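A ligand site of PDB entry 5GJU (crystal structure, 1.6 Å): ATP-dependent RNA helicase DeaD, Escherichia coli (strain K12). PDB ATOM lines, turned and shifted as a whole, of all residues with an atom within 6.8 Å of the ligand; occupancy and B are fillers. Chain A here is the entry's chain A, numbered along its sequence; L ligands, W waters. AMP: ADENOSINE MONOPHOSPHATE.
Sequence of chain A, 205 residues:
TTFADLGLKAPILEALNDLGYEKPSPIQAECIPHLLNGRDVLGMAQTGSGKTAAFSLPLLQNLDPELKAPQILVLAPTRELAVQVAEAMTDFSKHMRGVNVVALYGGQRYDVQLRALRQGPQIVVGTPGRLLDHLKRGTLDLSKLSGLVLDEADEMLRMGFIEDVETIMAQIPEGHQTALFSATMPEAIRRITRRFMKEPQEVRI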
ATOM      1  N   PHE A   3      -9.809   4.016 -13.634  1.00  0.00           N
ATOM      2  CA  PHE A   3     -11.154   3.861 -13.083  1.00  0.00           C
ATOM      3  C   PHE A   3     -11.273   4.525 -11.731  1.00  0.00           C
ATOM      4  O   PHE A   3     -12.321   5.099 -11.419  1.00  0.00           O
ATOM      5  CB  PHE A   3     -11.537   2.387 -13.008  1.00  0.00           C
ATOM      6  CG  PHE A   3     -11.961   1.811 -14.342  1.00  0.00           C
ATOM      7  CD1 PHE A   3     -13.184   2.162 -14.917  1.00  0.00           C
ATOM      8  CD2 PHE A   3     -11.137   0.953 -15.023  1.00  0.00           C
ATOM      9  CE1 PHE A   3     -13.576   1.625 -16.124  1.00  0.00           C
ATOM     10  CE2 PHE A   3     -11.536   0.414 -16.237  1.00  0.00           C
ATOM     11  CZ  PHE A   3     -12.749   0.760 -16.790  1.00  0.00           C
ATOM     12  N   LEU A  16     -13.360  -4.984 -11.513  1.00  0.00           N
ATOM     13  CA  LEU A  16     -12.748  -4.636 -12.782  1.00  0.00           C
ATOM     14  C   LEU A  16     -11.407  -5.331 -12.937  1.00  0.00           C
ATOM     15  O   LEU A  16     -11.056  -5.782 -14.022  1.00  0.00           O
ATOM     16  CB  LEU A  16     -12.584  -3.113 -12.891  1.00  0.00           C
ATOM     17  CG  LEU A  16     -13.902  -2.369 -12.908  1.00  0.00           C
ATOM     18  CD1 LEU A  16     -13.677  -0.876 -12.987  1.00  0.00           C
ATOM     19  CD2 LEU A  16     -14.776  -2.839 -14.070  1.00  0.00           C
ATOM     20  N   LEU A  19     -11.961  -8.843 -13.877  1.00  0.00           N
ATOM     21  CA  LEU A  19     -12.368  -8.910 -15.283  1.00  0.00           C
ATOM     22  C   LEU A  19     -11.245  -8.609 -16.249  1.00  0.00           C
ATOM     23  O   LEU A  19     -11.367  -8.919 -17.435  1.00  0.00           O
ATOM     24  CB  LEU A  19     -13.524  -7.928 -15.539  1.00  0.00           C
ATOM     25  CG  LEU A  19     -14.865  -8.351 -14.947  1.00  0.00           C
ATOM     26  CD1 LEU A  19     -15.920  -7.271 -15.212  1.00  0.00           C
ATOM     27  CD2 LEU A  19     -15.332  -9.696 -15.471  1.00  0.00           C
ATOM     28  N   GLY A  20     -10.156  -8.029 -15.777  1.00  0.00           N
ATOM     29  CA  GLY A  20      -9.066  -7.699 -16.644  1.00  0.00           C
ATOM     30  C   GLY A  20      -9.227  -6.386 -17.375  1.00  0.00           C
ATOM     31  O   GLY A  20      -8.559  -6.175 -18.382  1.00  0.00           O
ATOM     32  N   TYR A  21     -10.103  -5.501 -16.898  1.00  0.00           N
ATOM     33  CA  TYR A  21     -10.206  -4.164 -17.480  1.00  0.00           C
ATOM     34  C   TYR A  21      -9.079  -3.308 -16.923  1.00  0.00           C
ATOM     35  O   TYR A  21      -9.039  -3.031 -15.722  1.00  0.00           O
ATOM     36  CB  TYR A  21     -11.529  -3.473 -17.151  1.00  0.00           C
ATOM     37  CG  TYR A  21     -12.791  -4.076 -17.726  1.00  0.00           C
ATOM     38  CD1 TYR A  21     -12.776  -5.305 -18.349  1.00  0.00           C
ATOM     39  CD2 TYR A  21     -14.004  -3.407 -17.643  1.00  0.00           C
ATOM     40  CE1 TYR A  21     -13.905  -5.855 -18.860  1.00  0.00           C
ATOM     41  CE2 TYR A  21     -15.162  -3.958 -18.152  1.00  0.00           C
ATOM     42  CZ  TYR A  21     -15.100  -5.190 -18.749  1.00  0.00           C
ATOM     43  OH  TYR A  21     -16.229  -5.759 -19.256  1.00  0.00           O
ATOM     44  N   GLU A  22      -8.211  -2.855 -17.810  1.00  0.00           N
ATOM     45  CA  GLU A  22      -7.052  -2.097 -17.396  1.00  0.00           C
ATOM     46  C   GLU A  22      -7.325  -0.602 -17.342  1.00  0.00           C
ATOM     47  O   GLU A  22      -6.869   0.067 -16.415  1.00  0.00           O
ATOM     48  CB  GLU A  22      -5.892  -2.385 -18.352  1.00  0.00           C
ATOM     49  CG  GLU A  22      -5.453  -3.862 -18.374  1.00  0.00           C
ATOM     50  CD  GLU A  22      -4.422  -4.210 -17.317  1.00  0.00           C
ATOM     51  OE1 GLU A  22      -4.002  -3.312 -16.558  1.00  0.00           O
ATOM     52  OE2 GLU A  22      -4.024  -5.398 -17.259  1.00  0.00           O
ATOM     53  N   LYS A  23      -8.002  -0.051 -18.329  1.00  0.00           N
ATOM     54  CA  LYS A  23      -8.283   1.375 -18.311  1.00  0.00           C
ATOM     55  C   LYS A  23      -9.658   1.667 -18.874  1.00  0.00           C
ATOM     56  O   LYS A  23     -10.182   0.903 -19.687  1.00  0.00           O
ATOM     57  CB  LYS A  23      -7.251   2.164 -19.110  1.00  0.00           C
ATOM     58  CG  LYS A  23      -7.180   1.769 -20.528  1.00  0.00           C
ATOM     59  CD  LYS A  23      -6.091   2.567 -21.254  1.00  0.00           C
ATOM     60  CE  LYS A  23      -6.622   3.913 -21.696  1.00  0.00           C
ATOM     61  NZ  LYS A  23      -5.543   4.747 -22.291  1.00  0.00           N
ATOM     62  N   PRO A  24     -10.237   2.804 -18.513  1.00  0.00           N
ATOM     63  CA  PRO A  24     -11.549   3.155 -19.058  1.00  0.00           C
ATOM     64  C   PRO A  24     -11.511   3.428 -20.548  1.00  0.00           C
ATOM     65  O   PRO A  24     -10.577   4.053 -21.063  1.00  0.00           O
ATOM     66  CB  PRO A  24     -11.931   4.437 -18.303  1.00  0.00           C
ATOM     67  CG  PRO A  24     -11.009   4.532 -17.191  1.00  0.00           C
ATOM     68  CD  PRO A  24      -9.775   3.774 -17.518  1.00  0.00           C
ATOM     69  N   SER A  25     -12.588   3.021 -21.232  1.00  0.00           N
ATOM     70  CA  SER A  25     -12.814   3.444 -22.597  1.00  0.00           C
ATOM     71  C   SER A  25     -13.283   4.882 -22.607  1.00  0.00           C
ATOM     72  O   SER A  25     -13.729   5.406 -21.587  1.00  0.00           O
ATOM     73  CB  SER A  25     -13.866   2.573 -23.259  1.00  0.00           C
ATOM     74  OG  SER A  25     -15.135   2.792 -22.700  1.00  0.00           O
ATOM     75  N   ILE A  27     -16.024   6.299 -23.661  1.00  0.00           N
ATOM     76  CA  ILE A  27     -17.432   6.526 -23.272  1.00  0.00           C
ATOM     77  C   ILE A  27     -17.559   6.352 -21.765  1.00  0.00           C
ATOM     78  O   ILE A  27     -18.384   7.030 -21.111  1.00  0.00           O
ATOM     79  CB  ILE A  27     -18.399   5.598 -24.039  1.00  0.00           C
ATOM     80  CG1 ILE A  27     -19.853   6.046 -23.851  1.00  0.00           C
ATOM     81  CG2 ILE A  27     -18.331   4.142 -23.574  1.00  0.00           C
ATOM     82  CD1 ILE A  27     -20.155   7.340 -24.579  1.00  0.00           C
ATOM     83  N   GLN A  28     -16.724   5.493 -21.193  1.00  0.00           N
ATOM     84  CA  GLN A  28     -16.720   5.286 -19.742  1.00  0.00           C
ATOM     85  C   GLN A  28     -16.142   6.503 -19.028  1.00  0.00           C
ATOM     86  O   GLN A  28     -16.702   6.984 -18.032  1.00  0.00           O
ATOM     87  CB  GLN A  28     -15.923   4.021 -19.444  1.00  0.00           C
ATOM     88  CG  GLN A  28     -16.649   2.747 -19.828  1.00  0.00           C
ATOM     89  CD  GLN A  28     -15.767   1.528 -19.989  1.00  0.00           C
ATOM     90  OE1 GLN A  28     -14.568   1.553 -19.672  1.00  0.00           O
ATOM     91  NE2 GLN A  28     -16.378   0.447 -20.475  1.00  0.00           N
ATOM     92  N   GLN A  46     -22.185   2.713 -29.463  1.00  0.00           N
ATOM     93  CA  GLN A  46     -22.696   1.401 -29.859  1.00  0.00           C
ATOM     94  C   GLN A  46     -21.864   0.300 -29.214  1.00  0.00           C
ATOM     95  O   GLN A  46     -20.866   0.558 -28.535  1.00  0.00           O
ATOM     96  CB  GLN A  46     -22.684   1.235 -31.386  1.00  0.00           C
ATOM     97  CG  GLN A  46     -21.304   1.073 -31.953  1.00  0.00           C
ATOM     98  CD  GLN A  46     -21.353   0.690 -33.421  1.00  0.00           C
ATOM     99  OE1 GLN A  46     -22.372   0.893 -34.093  1.00  0.00           O
ATOM    100  NE2 GLN A  46     -20.254   0.122 -33.928  1.00  0.00           N
ATOM    101  N   THR A  47     -22.281  -0.957 -29.420  1.00  0.00           N
ATOM    102  CA  THR A  47     -21.590  -2.066 -28.774  1.00  0.00           C
ATOM    103  C   THR A  47     -20.135  -2.031 -29.201  1.00  0.00           C
ATOM    104  O   THR A  47     -19.793  -1.664 -30.333  1.00  0.00           O
ATOM    105  CB  THR A  47     -22.238  -3.409 -29.122  1.00  0.00           C
ATOM    106  OG1 THR A  47     -23.528  -3.494 -28.496  1.00  0.00           O
ATOM    107  CG2 THR A  47     -21.366  -4.596 -28.614  1.00  0.00           C
ATOM    108  N   GLY A  48     -19.274  -2.400 -28.284  1.00  0.00           N
ATOM    109  CA  GLY A  48     -17.869  -2.335 -28.495  1.00  0.00           C
ATOM    110  C   GLY A  48     -17.239  -1.136 -27.840  1.00  0.00           C
ATOM    111  O   GLY A  48     -16.073  -1.195 -27.473  1.00  0.00           O
ATOM    112  N   SER A  49     -18.009  -0.062 -27.629  1.00  0.00           N
ATOM    113  CA  SER A  49     -17.504   1.153 -27.002  1.00  0.00           C
ATOM    114  C   SER A  49     -17.247   0.974 -25.502  1.00  0.00           C
ATOM    115  O   SER A  49     -16.483   1.738 -24.921  1.00  0.00           O
ATOM    116  CB  SER A  49     -18.498   2.315 -27.188  1.00  0.00           C
ATOM    117  OG  SER A  49     -19.733   2.000 -26.549  1.00  0.00           O
ATOM    118  N   GLY A  50     -17.917   0.024 -24.863  1.00  0.00           N
ATOM    119  CA  GLY A  50     -17.913  -0.096 -23.438  1.00  0.00           C
ATOM    120  C   GLY A  50     -19.085   0.571 -22.771  1.00  0.00           C
ATOM    121  O   GLY A  50     -18.988   0.937 -21.601  1.00  0.00           O
ATOM    122  N   LYS A  51     -20.204   0.698 -23.476  1.00  0.00           N
ATOM    123  CA  LYS A  51     -21.355   1.405 -22.927  1.00  0.00           C
ATOM    124  C   LYS A  51     -21.959   0.683 -21.740  1.00  0.00           C
ATOM    125  O   LYS A  51     -22.493   1.320 -20.837  1.00  0.00           O
ATOM    126  CB  LYS A  51     -22.398   1.633 -24.016  1.00  0.00           C
ATOM    127  CG  LYS A  51     -22.803   0.388 -24.726  1.00  0.00           C
ATOM    128  CD  LYS A  51     -23.894   0.653 -25.716  1.00  0.00           C
ATOM    129  CE  LYS A  51     -24.179  -0.610 -26.506  1.00  0.00           C
ATOM    130  NZ  LYS A  51     -25.568  -0.963 -26.411  1.00  0.00           N
ATOM    131  N   THR A  52     -21.876  -0.653 -21.701  1.00  0.00           N
ATOM    132  CA  THR A  52     -22.486  -1.367 -20.573  1.00  0.00           C
ATOM    133  C   THR A  52     -21.862  -0.953 -19.246  1.00  0.00           C
ATOM    134  O   THR A  52     -22.568  -0.623 -18.284  1.00  0.00           O
ATOM    135  CB  THR A  52     -22.360  -2.889 -20.760  1.00  0.00           C
ATOM    136  OG1 THR A  52     -22.921  -3.264 -22.014  1.00  0.00           O
ATOM    137  CG2 THR A  52     -23.126  -3.607 -19.696  1.00  0.00           C
ATOM    138  N   ALA A  53     -20.535  -0.953 -19.146  1.00  0.00           N
ATOM    139  CA  ALA A  53     -19.894  -0.506 -17.914  1.00  0.00           C
ATOM    140  C   ALA A  53     -20.127   0.988 -17.682  1.00  0.00           C
ATOM    141  O   ALA A  53     -20.226   1.422 -16.515  1.00  0.00           O
ATOM    142  CB  ALA A  53     -18.409  -0.829 -17.950  1.00  0.00           C
ATOM    143  N   ALA A  54     -20.213   1.776 -18.760  1.00  0.00           N
ATOM    144  CA  ALA A  54     -20.439   3.220 -18.620  1.00  0.00           C
ATOM    145  C   ALA A  54     -21.701   3.520 -17.817  1.00  0.00           C
ATOM    146  O   ALA A  54     -21.688   4.435 -16.993  1.00  0.00           O
ATOM    147  CB  ALA A  54     -20.502   3.910 -19.991  1.00  0.00           C
ATOM    148  N   PHE A  55     -22.796   2.811 -18.066  1.00  0.00           N
ATOM    149  CA  PHE A  55     -23.981   3.039 -17.241  1.00  0.00           C
ATOM    150  C   PHE A  55     -24.008   2.155 -15.994  1.00  0.00           C
ATOM    151  O   PHE A  55     -24.569   2.558 -14.974  1.00  0.00           O
ATOM    152  CB  PHE A  55     -25.302   2.911 -18.025  1.00  0.00           C
ATOM    153  CG  PHE A  55     -25.593   1.548 -18.649  1.00  0.00           C
ATOM    154  CD1 PHE A  55     -26.052   0.475 -17.881  1.00  0.00           C
ATOM    155  CD2 PHE A  55     -25.528   1.388 -20.014  1.00  0.00           C
ATOM    156  CE1 PHE A  55     -26.362  -0.753 -18.487  1.00  0.00           C
ATOM    157  CE2 PHE A  55     -25.839   0.170 -20.623  1.00  0.00           C
ATOM    158  CZ  PHE A  55     -26.269  -0.889 -19.846  1.00  0.00           C
ATOM    159  N   LEU A  81     -29.273  -9.346 -25.478  1.00  0.00           N
ATOM    160  CA  LEU A  81     -28.638  -8.212 -24.795  1.00  0.00           C
ATOM    161  C   LEU A  81     -29.065  -8.139 -23.327  1.00  0.00           C
ATOM    162  O   LEU A  81     -28.243  -7.815 -22.463  1.00  0.00           O
ATOM    163  CB  LEU A  81     -28.973  -6.883 -25.491  1.00  0.00           C
ATOM    164  CG  LEU A  81     -28.227  -5.637 -24.995  1.00  0.00           C
ATOM    165  CD1 LEU A  81     -26.710  -5.841 -25.008  1.00  0.00           C
ATOM    166  CD2 LEU A  81     -28.605  -4.463 -25.887  1.00  0.00           C
ATOM    167  N   GLN A  84     -26.889 -10.563 -21.602  1.00  0.00           N
ATOM    168  CA  GLN A  84     -25.500 -10.105 -21.582  1.00  0.00           C
ATOM    169  C   GLN A  84     -25.296  -9.002 -20.548  1.00  0.00           C
ATOM    170  O   GLN A  84     -24.282  -8.979 -19.821  1.00  0.00           O
ATOM    171  CB  GLN A  84     -25.071  -9.588 -22.964  1.00  0.00           C
ATOM    172  CG  GLN A  84     -23.633  -8.990 -23.028  1.00  0.00           C
ATOM    173  CD  GLN A  84     -23.571  -7.500 -23.520  1.00  0.00           C
ATOM    174  OE1 GLN A  84     -23.738  -7.211 -24.711  1.00  0.00           O
ATOM    175  NE2 GLN A  84     -23.291  -6.565 -22.581  1.00  0.00           N
ATOM    176  N   PHE A  92     -19.747  -7.073 -12.369  1.00  0.00           N
ATOM    177  CA  PHE A  92     -19.322  -5.833 -11.746  1.00  0.00           C
ATOM    178  C   PHE A  92     -19.640  -5.780 -10.262  1.00  0.00           C
ATOM    179  O   PHE A  92     -18.970  -5.071  -9.516  1.00  0.00           O
ATOM    180  CB  PHE A  92     -19.984  -4.622 -12.409  1.00  0.00           C
ATOM    181  CG  PHE A  92     -19.746  -4.498 -13.894  1.00  0.00           C
ATOM    182  CD1 PHE A  92     -18.543  -4.859 -14.475  1.00  0.00           C
ATOM    183  CD2 PHE A  92     -20.752  -3.985 -14.704  1.00  0.00           C
ATOM    184  CE1 PHE A  92     -18.352  -4.704 -15.846  1.00  0.00           C
ATOM    185  CE2 PHE A  92     -20.574  -3.841 -16.072  1.00  0.00           C
ATOM    186  CZ  PHE A  92     -19.392  -4.202 -16.644  1.00  0.00           C
HETATM  187  P   AMP L   1     -20.029  -3.124 -24.586  1.00  0.00           P
HETATM  188  O1P AMP L   1     -19.662  -2.037 -25.552  1.00  0.00           O
HETATM  189  O2P AMP L   1     -20.924  -4.192 -25.207  1.00  0.00           O
HETATM  190  O3P AMP L   1     -20.424  -2.535 -23.258  1.00  0.00           O
HETATM  191  O5' AMP L   1     -18.665  -3.878 -24.281  1.00  0.00           O
HETATM  192  C5' AMP L   1     -17.885  -4.369 -25.355  1.00  0.00           C
HETATM  193  C4' AMP L   1     -16.815  -5.325 -24.886  1.00  0.00           C
HETATM  194  O4' AMP L   1     -15.724  -4.581 -24.317  1.00  0.00           O
HETATM  195  C3' AMP L   1     -17.225  -6.369 -23.845  1.00  0.00           C
HETATM  196  O3' AMP L   1     -16.596  -7.622 -24.186  1.00  0.00           O
HETATM  197  C2' AMP L   1     -16.618  -5.839 -22.548  1.00  0.00           C
HETATM  198  O2' AMP L   1     -16.266  -6.810 -21.601  1.00  0.00           O
HETATM  199  C1' AMP L   1     -15.374  -5.120 -23.054  1.00  0.00           C
HETATM  200  N9  AMP L   1     -14.940  -3.986 -22.251  1.00  0.00           N
HETATM  201  C8  AMP L   1     -15.751  -2.980 -21.856  1.00  0.00           C
HETATM  202  N7  AMP L   1     -15.054  -2.035 -21.212  1.00  0.00           N
HETATM  203  C5  AMP L   1     -13.762  -2.429 -21.229  1.00  0.00           C
HETATM  204  C6  AMP L   1     -12.524  -1.889 -20.704  1.00  0.00           C
HETATM  205  N6  AMP L   1     -12.543  -0.720 -20.076  1.00  0.00           N
HETATM  206  N1  AMP L   1     -11.406  -2.585 -20.889  1.00  0.00           N
HETATM  207  C2  AMP L   1     -11.394  -3.756 -21.523  1.00  0.00           C
HETATM  208  N3  AMP L   1     -12.486  -4.342 -22.023  1.00  0.00           N
HETATM  209  C4  AMP L   1     -13.698  -3.725 -21.893  1.00  0.00           C
HETATM  210  O   HOH W   1     -23.456  -4.247 -25.625  1.00  0.00           O
HETATM  211  O   HOH W   2     -18.884  -2.300 -21.007  1.00  0.00           O
HETATM  212  O   HOH W   3      -8.820  -1.983 -20.518  1.00  0.00           O
HETATM  213  O   HOH W   4     -13.698  -8.099 -24.606  1.00  0.00           O
HETATM  214  O   HOH W   5     -20.311  -6.802 -25.380  1.00  0.00           O
HETATM  215  O   HOH W   6      -8.744  -5.953 -21.008  1.00  0.00           O
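N of Tyr 21 lies within hydrogen-bond range of O of Leu 16 (3.0 Å). NE2 of Gln 28 sits at hydrogen-bond distance from O of Gly 50, at 2.9 Å. OG1 of Thr 52 sits at hydrogen-bond distance from NE2 of Gln 84. The backbone NH (N) of Ser 25 is in hydrogen-bond range of the side-chain amide oxygen (OE1) of Gln 28, 2.9 Å away. OG of Ser 49 is in hydrogen-bond range of N of Lys 51 (3.4 Å). The backbone carbonyl oxygen (O) of Ser 49 is in hydrogen-bond range of the side-chain hydroxyl (OG) of Ser 25 (2.8 Å). OG of Ser 49 is in hydrogen-bond range of O of Gln 46.
An oxygen (O2') of the ligand lies within hydrogen-bond range of the side-chain hydroxyl of Tyr 21. The backbone NH (N) of Gly 48 is in hydrogen-bond range of an oxygen (O1P) of the ligand. An oxygen (O1P) of the ligand is in hydrogen-bond range of the backbone NH of Gly 50 (2.8 Å). N of Thr 52 lies within hydrogen-bond range of O3P of the ligand, 2.8 Å away. An oxygen (O3P) of the ligand lies within hydrogen-bond range of the side-chain hydroxyl (OG1) of Thr 52 (2.9 Å). N6 of the ligand is in hydrogen-bond range of O of Lys 23 (2.9 Å). NE2 of Gln 28 lies within hydrogen-bond range of N7 of the ligand (2.9 Å). N of Lys 51 is in hydrogen-bond range of O3P of the ligand (3.2 Å). N of Ser 49 is in hydrogen-bond range of O1P of the ligand (3.3 Å).
CZ of Phe 3 touches N6 of the ligand (3.6 Å). Ser 25 touches the ligand (N to N6, 3.9 Å). CG2 of Thr 47 touches O2P of the ligand, 3.5 Å away. Hydrophobic or aromatic side chains within 4 Å of the ligand: Phe 3 and Tyr 21. Of the 24 residues printed, 11 come within 4 Å of the ligand.
Water W1 lies within hydrogen-bond range of O2P of the ligand (2.6 Å), OG1 of Thr 47 (3.0 Å) and OE1 of Gln 84 (3.1 Å). Water W3 lies within hydrogen-bond range of N1 of the ligand (2.7 Å), N of Glu 22 (2.9 Å) and N of Lys 23 (3.0 Å). Water W2 lies within hydrogen-bond range of an oxygen (O3P) of the ligand, the backbone NH (N) of Ala 53, the backbone carbonyl oxygen (O) of Gly 50 and the backbone NH (N) of Thr 52.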
